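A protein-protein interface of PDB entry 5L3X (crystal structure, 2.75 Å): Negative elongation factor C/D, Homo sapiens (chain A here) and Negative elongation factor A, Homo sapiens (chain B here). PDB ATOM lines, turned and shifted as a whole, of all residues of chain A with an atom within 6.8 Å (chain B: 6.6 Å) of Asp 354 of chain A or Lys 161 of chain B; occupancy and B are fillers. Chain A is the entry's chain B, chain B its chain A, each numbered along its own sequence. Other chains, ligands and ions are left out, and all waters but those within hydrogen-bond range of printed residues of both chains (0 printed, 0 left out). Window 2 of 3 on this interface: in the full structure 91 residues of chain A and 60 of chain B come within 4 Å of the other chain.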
ATOM      1  N   VAL A 349      34.354  11.615  -7.019  1.00  0.00           N
ATOM      2  CA  VAL A 349      34.007  10.819  -5.849  1.00  0.00           C
ATOM      3  C   VAL A 349      34.545  11.470  -4.581  1.00  0.00           C
ATOM      4  O   VAL A 349      33.822  11.632  -3.597  1.00  0.00           O
ATOM      5  CB  VAL A 349      34.554   9.386  -5.972  1.00  0.00           C
ATOM      6  CG1 VAL A 349      34.438   8.652  -4.649  1.00  0.00           C
ATOM      7  CG2 VAL A 349      33.828   8.632  -7.082  1.00  0.00           C
ATOM      8  N   THR A 350      35.818  11.852  -4.625  1.00  0.00           N
ATOM      9  CA  THR A 350      36.483  12.512  -3.506  1.00  0.00           C
ATOM     10  C   THR A 350      35.750  13.772  -3.057  1.00  0.00           C
ATOM     11  O   THR A 350      35.465  13.946  -1.870  1.00  0.00           O
ATOM     12  CB  THR A 350      37.931  12.895  -3.866  1.00  0.00           C
ATOM     13  OG1 THR A 350      38.665  11.720  -4.227  1.00  0.00           O
ATOM     14  CG2 THR A 350      38.611  13.569  -2.687  1.00  0.00           C
ATOM     15  N   GLU A 351      35.443  14.642  -4.015  1.00  0.00           N
ATOM     16  CA  GLU A 351      34.819  15.923  -3.713  1.00  0.00           C
ATOM     17  C   GLU A 351      33.400  15.762  -3.180  1.00  0.00           C
ATOM     18  O   GLU A 351      32.988  16.484  -2.274  1.00  0.00           O
ATOM     19  CB  GLU A 351      34.817  16.821  -4.953  1.00  0.00           C
ATOM     20  CG  GLU A 351      36.195  17.337  -5.343  1.00  0.00           C
ATOM     21  CD  GLU A 351      36.762  18.306  -4.322  1.00  0.00           C
ATOM     22  OE1 GLU A 351      36.045  19.254  -3.938  1.00  0.00           O
ATOM     23  OE2 GLU A 351      37.924  18.117  -3.900  1.00  0.00           O
ATOM     24  N   VAL A 352      32.654  14.815  -3.740  1.00  0.00           N
ATOM     25  CA  VAL A 352      31.284  14.576  -3.298  1.00  0.00           C
ATOM     26  C   VAL A 352      31.256  13.979  -1.893  1.00  0.00           C
ATOM     27  O   VAL A 352      30.460  14.394  -1.049  1.00  0.00           O
ATOM     28  CB  VAL A 352      30.528  13.644  -4.273  1.00  0.00           C
ATOM     29  CG1 VAL A 352      29.258  13.112  -3.635  1.00  0.00           C
ATOM     30  CG2 VAL A 352      30.200  14.380  -5.561  1.00  0.00           C
ATOM     31  N   LEU A 353      32.139  13.020  -1.635  1.00  0.00           N
ATOM     32  CA  LEU A 353      32.183  12.357  -0.336  1.00  0.00           C
ATOM     33  C   LEU A 353      32.734  13.269   0.755  1.00  0.00           C
ATOM     34  O   LEU A 353      32.656  12.945   1.940  1.00  0.00           O
ATOM     35  CB  LEU A 353      33.016  11.077  -0.419  1.00  0.00           C
ATOM     36  CG  LEU A 353      32.261   9.858  -0.954  1.00  0.00           C
ATOM     37  CD1 LEU A 353      33.205   8.689  -1.166  1.00  0.00           C
ATOM     38  CD2 LEU A 353      31.136   9.480  -0.002  1.00  0.00           C
ATOM     39  N   ASP A 354      33.282  14.410   0.351  1.00  0.00           N
ATOM     40  CA  ASP A 354      33.852  15.360   1.295  1.00  0.00           C
ATOM     41  C   ASP A 354      32.793  16.323   1.833  1.00  0.00           C
ATOM     42  O   ASP A 354      33.043  17.054   2.792  1.00  0.00           O
ATOM     43  CB  ASP A 354      34.991  16.145   0.632  1.00  0.00           C
ATOM     44  CG  ASP A 354      36.126  16.459   1.593  1.00  0.00           C
ATOM     45  OD1 ASP A 354      37.300  16.363   1.176  1.00  0.00           O
ATOM     46  OD2 ASP A 354      35.848  16.802   2.761  1.00  0.00           O
ATOM     47  N   VAL A 355      31.611  16.323   1.222  1.00  0.00           N
ATOM     48  CA  VAL A 355      30.573  17.280   1.606  1.00  0.00           C
ATOM     49  C   VAL A 355      29.220  16.647   1.953  1.00  0.00           C
ATOM     50  O   VAL A 355      28.338  17.327   2.476  1.00  0.00           O
ATOM     51  CB  VAL A 355      30.341  18.330   0.492  1.00  0.00           C
ATOM     52  CG1 VAL A 355      31.612  19.135   0.241  1.00  0.00           C
ATOM     53  CG2 VAL A 355      29.860  17.666  -0.788  1.00  0.00           C
ATOM     54  N   ILE A 356      29.047  15.358   1.672  1.00  0.00           N
ATOM     55  CA  ILE A 356      27.778  14.703   1.989  1.00  0.00           C
ATOM     56  C   ILE A 356      27.864  13.863   3.260  1.00  0.00           C
ATOM     57  O   ILE A 356      28.951  13.488   3.701  1.00  0.00           O
ATOM     58  CB  ILE A 356      27.282  13.808   0.832  1.00  0.00           C
ATOM     59  CG1 ILE A 356      28.171  12.574   0.667  1.00  0.00           C
ATOM     60  CG2 ILE A 356      27.194  14.605  -0.460  1.00  0.00           C
ATOM     61  CD1 ILE A 356      27.639  11.581  -0.349  1.00  0.00           C
ATOM     62  N   ALA A 357      26.704  13.577   3.840  1.00  0.00           N
ATOM     63  CA  ALA A 357      26.608  12.843   5.097  1.00  0.00           C
ATOM     64  C   ALA A 357      25.225  12.209   5.217  1.00  0.00           C
ATOM     65  O   ALA A 357      24.282  12.668   4.571  1.00  0.00           O
ATOM     66  CB  ALA A 357      26.881  13.772   6.276  1.00  0.00           C
ATOM     67  N   PRO A 358      25.099  11.146   6.034  1.00  0.00           N
ATOM     68  CA  PRO A 358      23.792  10.524   6.282  1.00  0.00           C
ATOM     69  C   PRO A 358      22.775  11.519   6.849  1.00  0.00           C
ATOM     70  O   PRO A 358      23.177  12.532   7.425  1.00  0.00           O
ATOM     71  CB  PRO A 358      24.110   9.418   7.301  1.00  0.00           C
ATOM     72  CG  PRO A 358      25.479   9.746   7.841  1.00  0.00           C
ATOM     73  CD  PRO A 358      26.186  10.413   6.708  1.00  0.00           C
ATOM     74  N   TYR A 360      21.105   9.037   3.818  1.00  0.00           N
ATOM     75  CA  TYR A 360      21.009   8.982   2.368  1.00  0.00           C
ATOM     76  C   TYR A 360      19.722   8.278   1.976  1.00  0.00           C
ATOM     77  O   TYR A 360      19.212   7.440   2.719  1.00  0.00           O
ATOM     78  CB  TYR A 360      22.203   8.250   1.751  1.00  0.00           C
ATOM     79  CG  TYR A 360      23.550   8.670   2.287  1.00  0.00           C
ATOM     80  CD1 TYR A 360      24.133   9.866   1.896  1.00  0.00           C
ATOM     81  CD2 TYR A 360      24.249   7.857   3.173  1.00  0.00           C
ATOM     82  CE1 TYR A 360      25.370  10.249   2.380  1.00  0.00           C
ATOM     83  CE2 TYR A 360      25.484   8.230   3.663  1.00  0.00           C
ATOM     84  CZ  TYR A 360      26.041   9.427   3.263  1.00  0.00           C
ATOM     85  OH  TYR A 360      27.271   9.801   3.749  1.00  0.00           O
ATOM     86  N   PRO A 389      36.818   8.137   4.007  1.00  0.00           N
ATOM     87  CA  PRO A 389      35.382   8.380   3.826  1.00  0.00           C
ATOM     88  C   PRO A 389      34.719   7.411   2.847  1.00  0.00           C
ATOM     89  O   PRO A 389      33.498   7.257   2.876  1.00  0.00           O
ATOM     90  CB  PRO A 389      35.343   9.808   3.282  1.00  0.00           C
ATOM     91  CG  PRO A 389      36.620   9.942   2.531  1.00  0.00           C
ATOM     92  CD  PRO A 389      37.638   9.132   3.292  1.00  0.00           C
ATOM     93  N   GLN B 159      22.719  15.093   3.425  1.00  0.00           N
ATOM     94  CA  GLN B 159      22.801  16.274   4.269  1.00  0.00           C
ATOM     95  C   GLN B 159      24.194  16.880   4.167  1.00  0.00           C
ATOM     96  O   GLN B 159      25.194  16.186   4.355  1.00  0.00           O
ATOM     97  CB  GLN B 159      22.468  15.920   5.720  1.00  0.00           C
ATOM     98  CG  GLN B 159      22.302  17.117   6.641  1.00  0.00           C
ATOM     99  CD  GLN B 159      21.718  16.737   7.989  1.00  0.00           C
ATOM    100  OE1 GLN B 159      21.482  17.594   8.840  1.00  0.00           O
ATOM    101  NE2 GLN B 159      21.477  15.444   8.189  1.00  0.00           N
ATOM    102  N   LEU B 160      24.256  18.171   3.856  1.00  0.00           N
ATOM    103  CA  LEU B 160      25.532  18.851   3.671  1.00  0.00           C
ATOM    104  C   LEU B 160      26.232  19.116   4.997  1.00  0.00           C
ATOM    105  O   LEU B 160      25.717  19.847   5.844  1.00  0.00           O
ATOM    106  CB  LEU B 160      25.333  20.169   2.918  1.00  0.00           C
ATOM    107  CG  LEU B 160      25.099  20.068   1.410  1.00  0.00           C
ATOM    108  CD1 LEU B 160      24.847  21.442   0.810  1.00  0.00           C
ATOM    109  CD2 LEU B 160      26.280  19.399   0.727  1.00  0.00           C
ATOM    110  N   LYS B 161      27.406  18.516   5.172  1.00  0.00           N
ATOM    111  CA  LYS B 161      28.219  18.771   6.355  1.00  0.00           C
ATOM    112  C   LYS B 161      29.001  20.074   6.183  1.00  0.00           C
ATOM    113  O   LYS B 161      29.116  20.868   7.116  1.00  0.00           O
ATOM    114  CB  LYS B 161      29.167  17.598   6.631  1.00  0.00           C
ATOM    115  CG  LYS B 161      30.009  17.168   5.434  1.00  0.00           C
ATOM    116  CD  LYS B 161      31.122  16.207   5.837  1.00  0.00           C
ATOM    117  CE  LYS B 161      30.563  14.900   6.368  1.00  0.00           C
ATOM    118  NZ  LYS B 161      31.634  13.888   6.578  1.00  0.00           N
ATOM    119  N   ARG B 162      29.527  20.289   4.981  1.00  0.00           N
ATOM    120  CA  ARG B 162      30.268  21.504   4.656  1.00  0.00           C
ATOM    121  C   ARG B 162      29.889  22.006   3.266  1.00  0.00           C
ATOM    122  O   ARG B 162      29.283  21.278   2.479  1.00  0.00           O
ATOM    123  CB  ARG B 162      31.780  21.259   4.727  1.00  0.00           C
ATOM    124  CG  ARG B 162      32.311  20.954   6.118  1.00  0.00           C
ATOM    125  CD  ARG B 162      33.794  20.623   6.079  1.00  0.00           C
ATOM    126  NE  ARG B 162      34.294  20.210   7.387  1.00  0.00           N
ATOM    127  CZ  ARG B 162      35.531  19.780   7.615  1.00  0.00           C
ATOM    128  NH1 ARG B 162      36.403  19.703   6.617  1.00  0.00           N
ATOM    129  NH2 ARG B 162      35.897  19.425   8.839  1.00  0.00           N
ATOM    130  N   LYS B 163      30.249  23.249   2.966  1.00  0.00           N
ATOM    131  CA  LYS B 163      30.003  23.806   1.643  1.00  0.00           C
ATOM    132  C   LYS B 163      31.123  23.408   0.685  1.00  0.00           C
ATOM    133  O   LYS B 163      32.287  23.335   1.080  1.00  0.00           O
ATOM    134  CB  LYS B 163      29.862  25.328   1.711  1.00  0.00           C
ATOM    135  CG  LYS B 163      28.484  25.827   1.296  1.00  0.00           C
ATOM    136  CD  LYS B 163      28.324  27.323   1.516  1.00  0.00           C
ATOM    137  CE  LYS B 163      26.910  27.775   1.185  1.00  0.00           C
ATOM    138  NZ  LYS B 163      26.719  29.235   1.409  1.00  0.00           N
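O of Gln 159 of chain B sits at hydrogen-bond distance from N of Ala 357 of chain A (3.1 Å). The side-chain amide nitrogen (NE2) of Gln 159 of chain B sits at hydrogen-bond distance from the backbone carbonyl oxygen (O) of Pro 358 of chain A, 3.5 Å away. The backbone NH (N) of Lys 161 of chain B is in hydrogen-bond range of the backbone carbonyl oxygen (O) of Val 355 of chain A (3.1 Å).
Among the printed residues, merely in contact across the chains: Asp 354 of chain A with Lys 161 of chain B, Val 355 of chain A with Gln 159 of chain B, Val 355 of chain A with Leu 160 of chain B, Val 355 of chain A with Arg 162 of chain B, Ile 356 of chain A with Gln 159 of chain B, Ile 356 of chain A with Lys 161 of chain B and Ala 357 of chain A with Lys 161 of chain B.
Asp 354 of chain A touches just one residue of chain B: Lys 161. Of the printed residues of chain B, Ala 357 of chain A touches Gln 159 and Lys 161. Of the printed residues of chain B, Pro 358 of chain A touches Gln 159. Of the printed residues of chain A, Leu 160 of chain B touches Val 355. Of chain A, only Asp 354, Val 355, Ile 356 and Ala 357 come within 4 Å of Lys 161 of chain B. Of the printed residues of chain A, Arg 162 of chain B touches Val 355 (3.7 Å). Lys 163 of chain B touches none of the printed residues of chain A.
Of the 12 printed residues of chain A, 5 touch a printed residue of chain B. Hydrophobic or aromatic side chains of chain A within 4 Å of the printed part of chain B: Val 355 and Ala 357. Printed residues of chain B that touch a printed residue of chain A: Gln 159, Leu 160, Lys 161 and Arg 162. Hydrophobic or aromatic side chains of chain B within 4 Å of the printed part of chain A: Leu 160. Among the printed residues, 10 pairs touch across the chains. Among the printed residues, no Asp or Glu carboxylate lies within 4 Å of a Lys or Arg side-chain nitrogen of the other chain.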
